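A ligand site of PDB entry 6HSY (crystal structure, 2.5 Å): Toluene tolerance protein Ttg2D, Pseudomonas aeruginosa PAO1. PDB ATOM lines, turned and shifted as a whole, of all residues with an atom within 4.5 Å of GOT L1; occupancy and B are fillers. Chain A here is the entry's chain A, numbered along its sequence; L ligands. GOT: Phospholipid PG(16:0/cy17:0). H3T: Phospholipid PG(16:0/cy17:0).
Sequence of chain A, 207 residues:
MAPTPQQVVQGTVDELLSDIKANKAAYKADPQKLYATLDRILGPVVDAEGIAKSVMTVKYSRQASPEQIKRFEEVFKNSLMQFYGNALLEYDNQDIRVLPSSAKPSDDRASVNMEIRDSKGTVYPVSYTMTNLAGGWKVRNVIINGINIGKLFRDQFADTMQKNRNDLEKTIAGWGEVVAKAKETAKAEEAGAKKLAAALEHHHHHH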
ATOM      1  N   VAL A  46      37.654  -0.754 -13.811  1.00  0.00           N
ATOM      2  CA  VAL A  46      37.318   0.248 -14.816  1.00  0.00           C
ATOM      3  C   VAL A  46      38.616   0.783 -15.409  1.00  0.00           C
ATOM      4  O   VAL A  46      39.536   1.161 -14.669  1.00  0.00           O
ATOM      5  CB  VAL A  46      36.476   1.398 -14.224  1.00  0.00           C
ATOM      6  CG1 VAL A  46      36.408   2.584 -15.182  1.00  0.00           C
ATOM      7  CG2 VAL A  46      35.076   0.901 -13.906  1.00  0.00           C
ATOM      8  N   ILE A  51      39.162   4.537 -21.268  1.00  0.00           N
ATOM      9  CA  ILE A  51      37.889   5.127 -21.672  1.00  0.00           C
ATOM     10  C   ILE A  51      38.087   6.590 -22.065  1.00  0.00           C
ATOM     11  O   ILE A  51      37.574   7.050 -23.093  1.00  0.00           O
ATOM     12  CB  ILE A  51      36.851   4.985 -20.534  1.00  0.00           C
ATOM     13  CG1 ILE A  51      36.502   3.507 -20.338  1.00  0.00           C
ATOM     14  CG2 ILE A  51      35.604   5.794 -20.830  1.00  0.00           C
ATOM     15  CD1 ILE A  51      35.686   3.231 -19.083  1.00  0.00           C
ATOM     16  N   PHE A  76      34.699  13.429 -15.875  1.00  0.00           N
ATOM     17  CA  PHE A  76      33.863  12.338 -16.352  1.00  0.00           C
ATOM     18  C   PHE A  76      33.337  11.502 -15.190  1.00  0.00           C
ATOM     19  O   PHE A  76      32.130  11.264 -15.073  1.00  0.00           O
ATOM     20  CB  PHE A  76      34.653  11.468 -17.327  1.00  0.00           C
ATOM     21  CG  PHE A  76      33.823  10.820 -18.402  1.00  0.00           C
ATOM     22  CD1 PHE A  76      32.464  10.599 -18.230  1.00  0.00           C
ATOM     23  CD2 PHE A  76      34.414  10.412 -19.588  1.00  0.00           C
ATOM     24  CE1 PHE A  76      31.716  10.002 -19.229  1.00  0.00           C
ATOM     25  CE2 PHE A  76      33.666   9.816 -20.588  1.00  0.00           C
ATOM     26  CZ  PHE A  76      32.313   9.612 -20.407  1.00  0.00           C
ATOM     27  N   LYS A  77      34.237  11.060 -14.298  1.00  0.00           N
ATOM     28  CA  LYS A  77      33.823  10.260 -13.150  1.00  0.00           C
ATOM     29  C   LYS A  77      32.853  11.038 -12.262  1.00  0.00           C
ATOM     30  O   LYS A  77      31.740  10.588 -11.990  1.00  0.00           O
ATOM     31  CB  LYS A  77      35.050   9.840 -12.331  1.00  0.00           C
ATOM     32  CG  LYS A  77      36.021   8.921 -13.044  1.00  0.00           C
ATOM     33  CD  LYS A  77      37.250   8.678 -12.181  1.00  0.00           C
ATOM     34  CE  LYS A  77      38.333   7.928 -12.919  1.00  0.00           C
ATOM     35  NZ  LYS A  77      39.507   7.634 -12.055  1.00  0.00           N
ATOM     36  N   LEU A  80      29.464  11.688 -13.748  1.00  0.00           N
ATOM     37  CA  LEU A  80      28.683  10.454 -13.841  1.00  0.00           C
ATOM     38  C   LEU A  80      28.064  10.090 -12.501  1.00  0.00           C
ATOM     39  O   LEU A  80      26.905   9.677 -12.443  1.00  0.00           O
ATOM     40  CB  LEU A  80      29.565   9.311 -14.356  1.00  0.00           C
ATOM     41  CG  LEU A  80      29.807   9.251 -15.865  1.00  0.00           C
ATOM     42  CD1 LEU A  80      30.888   8.244 -16.204  1.00  0.00           C
ATOM     43  CD2 LEU A  80      28.518   8.905 -16.592  1.00  0.00           C
ATOM     44  N   TYR A  84      24.091  10.418 -12.046  1.00  0.00           N
ATOM     45  CA  TYR A  84      23.588   9.070 -12.231  1.00  0.00           C
ATOM     46  C   TYR A  84      23.921   8.138 -11.078  1.00  0.00           C
ATOM     47  O   TYR A  84      23.709   6.923 -11.199  1.00  0.00           O
ATOM     48  CB  TYR A  84      24.113   8.480 -13.549  1.00  0.00           C
ATOM     49  CG  TYR A  84      23.798   9.331 -14.767  1.00  0.00           C
ATOM     50  CD1 TYR A  84      22.525   9.348 -15.313  1.00  0.00           C
ATOM     51  CD2 TYR A  84      24.777  10.111 -15.367  1.00  0.00           C
ATOM     52  CE1 TYR A  84      22.230  10.105 -16.422  1.00  0.00           C
ATOM     53  CE2 TYR A  84      24.494  10.879 -16.483  1.00  0.00           C
ATOM     54  CZ  TYR A  84      23.211  10.876 -17.004  1.00  0.00           C
ATOM     55  OH  TYR A  84      22.919  11.643 -18.110  1.00  0.00           O
ATOM     56  N   ILE A 116      18.620  -6.597 -17.750  1.00  0.00           N
ATOM     57  CA  ILE A 116      18.127  -5.959 -16.535  1.00  0.00           C
ATOM     58  C   ILE A 116      16.608  -5.987 -16.601  1.00  0.00           C
ATOM     59  O   ILE A 116      16.001  -5.260 -17.407  1.00  0.00           O
ATOM     60  CB  ILE A 116      18.648  -4.524 -16.375  1.00  0.00           C
ATOM     61  CG1 ILE A 116      20.171  -4.524 -16.302  1.00  0.00           C
ATOM     62  CG2 ILE A 116      18.036  -3.878 -15.134  1.00  0.00           C
ATOM     63  CD1 ILE A 116      20.796  -3.140 -16.187  1.00  0.00           C
ATOM     64  N   TYR A 124      15.988  -4.564 -20.771  1.00  0.00           N
ATOM     65  CA  TYR A 124      16.888  -3.852 -21.657  1.00  0.00           C
ATOM     66  C   TYR A 124      18.244  -4.526 -21.605  1.00  0.00           C
ATOM     67  O   TYR A 124      18.736  -4.835 -20.511  1.00  0.00           O
ATOM     68  CB  TYR A 124      17.040  -2.385 -21.236  1.00  0.00           C
ATOM     69  CG  TYR A 124      15.752  -1.680 -20.863  1.00  0.00           C
ATOM     70  CD1 TYR A 124      14.883  -1.208 -21.843  1.00  0.00           C
ATOM     71  CD2 TYR A 124      15.414  -1.478 -19.532  1.00  0.00           C
ATOM     72  CE1 TYR A 124      13.708  -0.561 -21.508  1.00  0.00           C
ATOM     73  CE2 TYR A 124      14.243  -0.827 -19.184  1.00  0.00           C
ATOM     74  CZ  TYR A 124      13.400  -0.371 -20.174  1.00  0.00           C
ATOM     75  OH  TYR A 124      12.226   0.272 -19.831  1.00  0.00           O
ATOM     76  N   VAL A 126      22.274  -4.812 -21.551  1.00  0.00           N
ATOM     77  CA  VAL A 126      23.441  -4.012 -21.203  1.00  0.00           C
ATOM     78  C   VAL A 126      24.669  -4.867 -21.433  1.00  0.00           C
ATOM     79  O   VAL A 126      24.735  -6.015 -20.972  1.00  0.00           O
ATOM     80  CB  VAL A 126      23.386  -3.520 -19.739  1.00  0.00           C
ATOM     81  CG1 VAL A 126      24.610  -2.684 -19.411  1.00  0.00           C
ATOM     82  CG2 VAL A 126      22.113  -2.723 -19.500  1.00  0.00           C
ATOM     83  N   TYR A 128      29.114  -5.060 -21.670  1.00  0.00           N
ATOM     84  CA  TYR A 128      30.364  -4.510 -21.174  1.00  0.00           C
ATOM     85  C   TYR A 128      31.502  -5.020 -22.043  1.00  0.00           C
ATOM     86  O   TYR A 128      31.692  -6.229 -22.162  1.00  0.00           O
ATOM     87  CB  TYR A 128      30.588  -4.900 -19.706  1.00  0.00           C
ATOM     88  CG  TYR A 128      29.515  -4.399 -18.769  1.00  0.00           C
ATOM     89  CD1 TYR A 128      28.310  -5.076 -18.659  1.00  0.00           C
ATOM     90  CD2 TYR A 128      29.699  -3.255 -18.007  1.00  0.00           C
ATOM     91  CE1 TYR A 128      27.323  -4.627 -17.800  1.00  0.00           C
ATOM     92  CE2 TYR A 128      28.725  -2.800 -17.147  1.00  0.00           C
ATOM     93  CZ  TYR A 128      27.534  -3.486 -17.054  1.00  0.00           C
ATOM     94  OH  TYR A 128      26.544  -3.046 -16.199  1.00  0.00           O
ATOM     95  N   ARG A 140      35.953  -1.262 -20.655  1.00  0.00           N
ATOM     96  CA  ARG A 140      36.439  -0.269 -21.601  1.00  0.00           C
ATOM     97  C   ARG A 140      35.315   0.450 -22.345  1.00  0.00           C
ATOM     98  O   ARG A 140      35.561   1.527 -22.891  1.00  0.00           O
ATOM     99  CB  ARG A 140      37.369  -0.918 -22.633  1.00  0.00           C
ATOM    100  CG  ARG A 140      38.119   0.067 -23.516  1.00  0.00           C
ATOM    101  CD  ARG A 140      38.946  -0.644 -24.560  1.00  0.00           C
ATOM    102  NE  ARG A 140      39.509   0.296 -25.527  1.00  0.00           N
ATOM    103  CZ  ARG A 140      38.824   0.865 -26.507  1.00  0.00           C
ATOM    104  NH1 ARG A 140      37.530   0.602 -26.665  1.00  0.00           N
ATOM    105  NH2 ARG A 140      39.422   1.705 -27.337  1.00  0.00           N
ATOM    106  N   ASN A 141      34.112  -0.103 -22.375  1.00  0.00           N
ATOM    107  CA  ASN A 141      32.987   0.518 -23.057  1.00  0.00           C
ATOM    108  C   ASN A 141      31.707  -0.150 -22.566  1.00  0.00           C
ATOM    109  O   ASN A 141      31.724  -1.301 -22.135  1.00  0.00           O
ATOM    110  CB  ASN A 141      33.122   0.387 -24.582  1.00  0.00           C
ATOM    111  CG  ASN A 141      32.038   1.142 -25.334  1.00  0.00           C
ATOM    112  OD1 ASN A 141      31.432   2.074 -24.803  1.00  0.00           O
ATOM    113  ND2 ASN A 141      31.806   0.740 -26.571  1.00  0.00           N
ATOM    114  N   VAL A 142      30.607   0.593 -22.638  1.00  0.00           N
ATOM    115  CA  VAL A 142      29.310   0.131 -22.177  1.00  0.00           C
ATOM    116  C   VAL A 142      28.281   0.399 -23.268  1.00  0.00           C
ATOM    117  O   VAL A 142      28.172   1.530 -23.757  1.00  0.00           O
ATOM    118  CB  VAL A 142      28.892   0.810 -20.858  1.00  0.00           C
ATOM    119  CG1 VAL A 142      27.513   0.327 -20.412  1.00  0.00           C
ATOM    120  CG2 VAL A 142      29.926   0.568 -19.776  1.00  0.00           C
ATOM    121  N   ILE A 144      24.170   0.090 -24.019  1.00  0.00           N
ATOM    122  CA  ILE A 144      22.897   0.000 -23.305  1.00  0.00           C
ATOM    123  C   ILE A 144      21.768   0.024 -24.320  1.00  0.00           C
ATOM    124  O   ILE A 144      21.575   1.039 -25.017  1.00  0.00           O
ATOM    125  CB  ILE A 144      22.735   1.153 -22.297  1.00  0.00           C
ATOM    126  CG1 ILE A 144      23.932   1.206 -21.350  1.00  0.00           C
ATOM    127  CG2 ILE A 144      21.448   0.987 -21.509  1.00  0.00           C
ATOM    128  CD1 ILE A 144      23.974   2.436 -20.467  1.00  0.00           C
ATOM    129  N   ASN A 145      21.033  -1.078 -24.407  1.00  0.00           N
ATOM    130  CA  ASN A 145      19.851  -1.169 -25.285  1.00  0.00           C
ATOM    131  C   ASN A 145      20.192  -0.716 -26.702  1.00  0.00           C
ATOM    132  O   ASN A 145      19.428   0.001 -27.343  1.00  0.00           O
ATOM    133  CB  ASN A 145      18.699  -0.357 -24.701  1.00  0.00           C
ATOM    134  CG  ASN A 145      17.377  -0.665 -25.383  1.00  0.00           C
ATOM    135  OD1 ASN A 145      17.241  -1.667 -26.088  1.00  0.00           O
ATOM    136  ND2 ASN A 145      16.377   0.179 -25.155  1.00  0.00           N
ATOM    137  N   ILE A 149      27.462   3.700 -25.649  1.00  0.00           N
ATOM    138  CA  ILE A 149      27.682   4.902 -24.839  1.00  0.00           C
ATOM    139  C   ILE A 149      29.058   5.479 -25.114  1.00  0.00           C
ATOM    140  O   ILE A 149      29.237   6.707 -25.118  1.00  0.00           O
ATOM    141  CB  ILE A 149      27.484   4.568 -23.340  1.00  0.00           C
ATOM    142  CG1 ILE A 149      26.162   3.827 -23.107  1.00  0.00           C
ATOM    143  CG2 ILE A 149      27.524   5.838 -22.515  1.00  0.00           C
ATOM    144  CD1 ILE A 149      24.932   4.589 -23.563  1.00  0.00           C
ATOM    145  N   GLY A 150      30.055   4.622 -25.337  1.00  0.00           N
ATOM    146  CA  GLY A 150      31.379   5.110 -25.653  1.00  0.00           C
ATOM    147  C   GLY A 150      31.394   5.965 -26.909  1.00  0.00           C
ATOM    148  O   GLY A 150      31.961   7.068 -26.919  1.00  0.00           O
ATOM    149  N   PHE A 153      29.623   9.478 -26.307  1.00  0.00           N
ATOM    150  CA  PHE A 153      30.528  10.485 -25.754  1.00  0.00           C
ATOM    151  C   PHE A 153      31.648  10.811 -26.729  1.00  0.00           C
ATOM    152  O   PHE A 153      32.151  11.944 -26.730  1.00  0.00           O
ATOM    153  CB  PHE A 153      31.093  10.014 -24.422  1.00  0.00           C
ATOM    154  CG  PHE A 153      30.093  10.029 -23.298  1.00  0.00           C
ATOM    155  CD1 PHE A 153      29.487  11.200 -22.906  1.00  0.00           C
ATOM    156  CD2 PHE A 153      29.764   8.857 -22.635  1.00  0.00           C
ATOM    157  CE1 PHE A 153      28.564  11.219 -21.875  1.00  0.00           C
ATOM    158  CE2 PHE A 153      28.847   8.861 -21.602  1.00  0.00           C
ATOM    159  CZ  PHE A 153      28.254  10.043 -21.216  1.00  0.00           C
ATOM    160  N   ALA A 182      23.599  13.417 -21.204  1.00  0.00           N
ATOM    161  CA  ALA A 182      23.842  12.194 -21.951  1.00  0.00           C
ATOM    162  C   ALA A 182      22.609  11.301 -22.004  1.00  0.00           C
ATOM    163  O   ALA A 182      22.404  10.579 -22.978  1.00  0.00           O
ATOM    164  CB  ALA A 182      25.009  11.427 -21.336  1.00  0.00           C
ATOM    165  N   LYS A 183      21.777  11.340 -20.960  1.00  0.00           N
ATOM    166  CA  LYS A 183      20.603  10.472 -20.915  1.00  0.00           C
ATOM    167  C   LYS A 183      19.584  10.869 -21.965  1.00  0.00           C
ATOM    168  O   LYS A 183      19.162  10.036 -22.785  1.00  0.00           O
ATOM    169  CB  LYS A 183      19.997  10.518 -19.516  1.00  0.00           C
ATOM    170  CG  LYS A 183      18.871   9.532 -19.254  1.00  0.00           C
ATOM    171  CD  LYS A 183      17.949  10.101 -18.183  1.00  0.00           C
ATOM    172  CE  LYS A 183      17.153   9.039 -17.471  1.00  0.00           C
ATOM    173  NZ  LYS A 183      16.139   9.702 -16.603  1.00  0.00           N
ATOM    174  N   ALA A 186      20.676  10.177 -25.345  1.00  0.00           N
ATOM    175  CA  ALA A 186      20.456   8.788 -25.732  1.00  0.00           C
ATOM    176  C   ALA A 186      19.004   8.525 -26.090  1.00  0.00           C
ATOM    177  O   ALA A 186      18.718   7.800 -27.047  1.00  0.00           O
ATOM    178  CB  ALA A 186      20.908   7.853 -24.613  1.00  0.00           C
ATOM    179  N   LYS A 187      18.072   9.104 -25.327  1.00  0.00           N
ATOM    180  CA  LYS A 187      16.656   8.921 -25.613  1.00  0.00           C
ATOM    181  C   LYS A 187      16.301   9.467 -26.992  1.00  0.00           C
ATOM    182  O   LYS A 187      15.664   8.776 -27.802  1.00  0.00           O
ATOM    183  CB  LYS A 187      15.806   9.606 -24.546  1.00  0.00           C
ATOM    184  CG  LYS A 187      15.991   9.044 -23.150  1.00  0.00           C
ATOM    185  CD  LYS A 187      15.494   7.608 -23.055  1.00  0.00           C
ATOM    186  CE  LYS A 187      15.625   7.068 -21.642  1.00  0.00           C
ATOM    187  NZ  LYS A 187      14.875   7.891 -20.672  1.00  0.00           N
ATOM    188  N   GLU A 190      17.369   7.354 -29.558  1.00  0.00           N
ATOM    189  CA  GLU A 190      16.683   6.064 -29.531  1.00  0.00           C
ATOM    190  C   GLU A 190      15.333   6.113 -30.234  1.00  0.00           C
ATOM    191  O   GLU A 190      14.874   5.092 -30.753  1.00  0.00           O
ATOM    192  CB  GLU A 190      16.494   5.601 -28.086  1.00  0.00           C
ATOM    193  CG  GLU A 190      16.736   4.109 -27.869  1.00  0.00           C
ATOM    194  CD  GLU A 190      16.776   3.738 -26.398  1.00  0.00           C
ATOM    195  OE1 GLU A 190      16.541   4.621 -25.553  1.00  0.00           O
ATOM    196  OE2 GLU A 190      17.043   2.557 -26.093  1.00  0.00           O
HETATM  197  C10 GOT L   1      25.237   0.462 -16.380  1.00  0.00           C
HETATM  198  C11 GOT L   1      26.412   1.155 -15.615  1.00  0.00           C
HETATM  199  C12 GOT L   1      27.831   0.565 -15.863  1.00  0.00           C
HETATM  200  C01 GOT L   1      16.831   3.436 -20.651  1.00  0.00           C
HETATM  201  C02 GOT L   1      17.593   2.249 -19.898  1.00  0.00           C
HETATM  202  C04 GOT L   1      18.990   1.767 -17.968  1.00  0.00           C
HETATM  203  C06 GOT L   1      20.522   2.043 -17.746  1.00  0.00           C
HETATM  204  C07 GOT L   1      21.229   1.045 -16.736  1.00  0.00           C
HETATM  205  C08 GOT L   1      22.697   0.623 -17.106  1.00  0.00           C
HETATM  206  C09 GOT L   1      23.814   1.049 -16.100  1.00  0.00           C
HETATM  207  C13 GOT L   1      29.007   1.259 -15.098  1.00  0.00           C
HETATM  208  C14 GOT L   1      30.437   1.060 -15.667  1.00  0.00           C
HETATM  209  C15 GOT L   1      31.510   2.014 -15.054  1.00  0.00           C
HETATM  210  C16 GOT L   1      32.275   2.916 -16.069  1.00  0.00           C
HETATM  211  C17 GOT L   1      32.935   4.194 -15.460  1.00  0.00           C
HETATM  212  C18 GOT L   1      33.539   5.181 -16.485  1.00  0.00           C
HETATM  213  C19 GOT L   1      34.525   6.225 -15.899  1.00  0.00           C
HETATM  214  C20 GOT L   1      35.156   7.159 -16.930  1.00  0.00           C
HETATM  215  C21 GOT L   1      16.829   3.181 -22.227  1.00  0.00           C
HETATM  216  C27 GOT L   1      11.744   2.137 -22.702  1.00  0.00           C
HETATM  217  C28 GOT L   1      10.731   1.713 -23.817  1.00  0.00           C
HETATM  218  C30 GOT L   1       9.314   2.372 -23.692  1.00  0.00           C
HETATM  219  C33 GOT L   1      18.620   5.064 -21.152  1.00  0.00           C
HETATM  220  C35 GOT L   1      20.029   4.644 -20.618  1.00  0.00           C
HETATM  221  C36 GOT L   1      21.199   5.560 -21.132  1.00  0.00           C
HETATM  222  C37 GOT L   1      21.596   6.757 -20.227  1.00  0.00           C
HETATM  223  C38 GOT L   1      22.991   7.389 -20.533  1.00  0.00           C
HETATM  224  C39 GOT L   1      23.919   7.640 -19.307  1.00  0.00           C
HETATM  225  C40 GOT L   1      25.255   6.845 -19.303  1.00  0.00           C
HETATM  226  C41 GOT L   1      25.874   6.617 -17.910  1.00  0.00           C
HETATM  227  C42 GOT L   1      26.222   5.194 -17.476  1.00  0.00           C
HETATM  228  C43 GOT L   1      27.324   4.977 -16.500  1.00  0.00           C
HETATM  229  C44 GOT L   1      27.536   4.500 -17.891  1.00  0.00           C
HETATM  230  C45 GOT L   1      28.571   5.168 -18.788  1.00  0.00           C
HETATM  231  C46 GOT L   1      30.056   4.885 -18.505  1.00  0.00           C
HETATM  232  C47 GOT L   1      31.051   5.575 -19.467  1.00  0.00           C
HETATM  233  C48 GOT L   1      30.973   5.098 -20.934  1.00  0.00           C
HETATM  234  C49 GOT L   1      32.151   5.532 -21.814  1.00  0.00           C
HETATM  235  C50 GOT L   1      32.768   4.402 -22.647  1.00  0.00           C
HETATM  236  O03 GOT L   1      18.277   2.717 -18.699  1.00  0.00           O
HETATM  237  O05 GOT L   1      18.446   0.792 -17.559  1.00  0.00           O
HETATM  238  O22 GOT L   1      15.757   2.406 -22.604  1.00  0.00           O
HETATM  239  O24 GOT L   1      14.322   3.821 -24.263  1.00  0.00           O
HETATM  240  O25 GOT L   1      13.881   3.937 -21.687  1.00  0.00           O
HETATM  241  O26 GOT L   1      13.046   1.891 -23.071  1.00  0.00           O
HETATM  242  O29 GOT L   1      11.251   2.157 -25.030  1.00  0.00           O
HETATM  243  O31 GOT L   1       8.660   2.191 -24.906  1.00  0.00           O
HETATM  244  O32 GOT L   1      17.485   4.726 -20.384  1.00  0.00           O
HETATM  245  O34 GOT L   1      18.468   5.646 -22.171  1.00  0.00           O
HETATM  246  P23 GOT L   1      14.221   3.180 -22.927  1.00  0.00           P
HETATM  247  C10 H3T L   2      25.482   4.313 -13.075  1.00  0.00           C
HETATM  248  C11 H3T L   2      26.589   5.360 -12.811  1.00  0.00           C
HETATM  249  C12 H3T L   2      27.918   4.789 -12.268  1.00  0.00           C
HETATM  250  C01 H3T L   2      17.399   4.614 -15.573  1.00  0.00           C
HETATM  251  C02 H3T L   2      17.853   5.880 -14.684  1.00  0.00           C
HETATM  252  C04 H3T L   2      19.977   6.001 -15.892  1.00  0.00           C
HETATM  253  C06 H3T L   2      21.289   5.917 -15.035  1.00  0.00           C
HETATM  254  C07 H3T L   2      22.114   4.595 -15.252  1.00  0.00           C
HETATM  255  C08 H3T L   2      23.070   4.228 -14.092  1.00  0.00           C
HETATM  256  C09 H3T L   2      24.565   4.585 -14.286  1.00  0.00           C
HETATM  257  C13 H3T L   2      29.037   5.819 -12.025  1.00  0.00           C
HETATM  258  C14 H3T L   2      30.459   5.402 -12.467  1.00  0.00           C
HETATM  259  C15 H3T L   2      31.574   5.809 -11.493  1.00  0.00           C
HETATM  260  C16 H3T L   2      33.002   5.413 -11.936  1.00  0.00           C
HETATM  261  C17 H3T L   2      33.917   4.851 -10.825  1.00  0.00           C
HETATM  262  C18 H3T L   2      35.232   4.232 -11.326  1.00  0.00           C
HETATM  263  C19 H3T L   2      36.502   4.985 -10.932  1.00  0.00           C
HETATM  264  C20 H3T L   2      37.716   4.700 -11.817  1.00  0.00           C
HETATM  265  C21 H3T L   2      16.716   5.114 -16.903  1.00  0.00           C
HETATM  266  C27 H3T L   2      13.866   7.122 -17.314  1.00  0.00           C
HETATM  267  C28 H3T L   2      12.634   8.056 -17.100  1.00  0.00           C
HETATM  268  C30 H3T L   2      11.742   8.232 -18.373  1.00  0.00           C
HETATM  269  C33 H3T L   2      16.939   3.064 -13.788  1.00  0.00           C
HETATM  270  C35 H3T L   2      17.701   1.719 -14.079  1.00  0.00           C
HETATM  271  C36 H3T L   2      18.929   1.479 -13.125  1.00  0.00           C
HETATM  272  C37 H3T L   2      19.546   0.051 -13.154  1.00  0.00           C
HETATM  273  C38 H3T L   2      21.103  -0.010 -13.148  1.00  0.00           C
HETATM  274  C39 H3T L   2      21.745  -1.155 -12.319  1.00  0.00           C
HETATM  275  C40 H3T L   2      22.566  -2.207 -13.129  1.00  0.00           C
HETATM  276  C41 H3T L   2      23.783  -2.807 -12.389  1.00  0.00           C
HETATM  277  C42 H3T L   2      24.770  -1.805 -11.790  1.00  0.00           C
HETATM  278  C43 H3T L   2      25.515  -0.894 -12.708  1.00  0.00           C
HETATM  279  C44 H3T L   2      26.298  -1.912 -11.961  1.00  0.00           C
HETATM  280  C45 H3T L   2      26.992  -3.040 -12.733  1.00  0.00           C
HETATM  281  C46 H3T L   2      28.378  -2.705 -13.265  1.00  0.00           C
HETATM  282  C47 H3T L   2      29.332  -3.875 -13.507  1.00  0.00           C
HETATM  283  C48 H3T L   2      30.698  -3.421 -14.079  1.00  0.00           C
HETATM  284  C49 H3T L   2      31.506  -4.503 -14.815  1.00  0.00           C
HETATM  285  C50 H3T L   2      32.906  -4.712 -14.230  1.00  0.00           C
HETATM  286  O03 H3T L   2      18.882   6.692 -15.340  1.00  0.00           O
HETATM  287  O05 H3T L   2      19.893   5.508 -16.974  1.00  0.00           O
HETATM  288  O22 H3T L   2      15.879   4.160 -17.446  1.00  0.00           O
HETATM  289  O24 H3T L   2      13.434   3.302 -16.997  1.00  0.00           O
HETATM  290  O25 H3T L   2      13.963   4.768 -19.100  1.00  0.00           O
HETATM  291  O26 H3T L   2      13.715   5.889 -16.731  1.00  0.00           O
HETATM  292  O29 H3T L   2      13.125   9.315 -16.767  1.00  0.00           O
HETATM  293  O31 H3T L   2      10.631   8.989 -18.022  1.00  0.00           O
HETATM  294  O32 H3T L   2      16.440   3.791 -14.873  1.00  0.00           O
HETATM  295  O34 H3T L   2      16.798   3.499 -12.705  1.00  0.00           O
HETATM  296  P23 H3T L   2      14.136   4.441 -17.652  1.00  0.00           P
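The side-chain carboxylate (OE2) of Glu 190 is in hydrogen-bond range of the side-chain amide nitrogen (ND2) of Asn 145 (2.6 Å).
The backbone NH (N) of Ile 149 lies within hydrogen-bond range of the backbone carbonyl oxygen (O) of Val 142 (3.0 Å).
The side-chain hydroxyl (OH) of Tyr 84 lies within hydrogen-bond range of the backbone NH (N) of Lys 183, at 3.1 Å.
O of Tyr 124 lies within hydrogen-bond range of N of Ile 116 (3.3 Å).
N of Gly 150 lies within hydrogen-bond range of OD1 of Asn 141 (2.9 Å).
An oxygen (O25) of H3T L2 lies close to an oxygen (O25) of GOT L1, at 2.7 Å.
Val 46 touches GOT L1 (CG1 to C17, 3.8 Å).
Ile 51 touches GOT L1 (CG2 to C49, 3.6 Å).
Leu 80 touches GOT L1.
Tyr 124 touches GOT L1.
Tyr 128 touches GOT L1 (CE2 to C12, 3.7 Å).
Asn 141 touches GOT L1.
Ile 149 touches GOT L1 (CG2 to C48, 3.9 Å).
Gly 150 touches GOT L1 (CA to C50, 3.4 Å).
CA of Lys 183 touches C37 of GOT L1, 3.9 Å away.
CE of Lys 187 touches O34 of GOT L1, 3.2 Å away.
Hydrophobic or aromatic side chains that line GOT L1: Val 46, Ile 51, Leu 80, Tyr 124, Tyr 128 and Ile 149.
12 residues have an atom within 4 Å of GOT L1: Val 46, Ile 51, Leu 80, Tyr 124, Tyr 128, Asn 141, Asn 145, Ile 149, Gly 150, Lys 183, Lys 187 and Glu 190.
The nearest printed residue that does not touch GOT L1 is Arg 140 (4.02 Å).
The side-chain amino group (NZ) of Lys 187 is in salt-bridge range of an oxygen (O25) of H3T L2, at 3.6 Å.
The side-chain amino group (NZ) of Lys 183 sits at hydrogen-bond distance from an oxygen (O29) of H3T L2 (3.0 Å).
The side-chain carboxylate of Glu 190 sits close to an oxygen (O24) of GOT L1.
ND2 of Asn 145 is in hydrogen-bond range of O22 of GOT L1 (3.4 Å).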
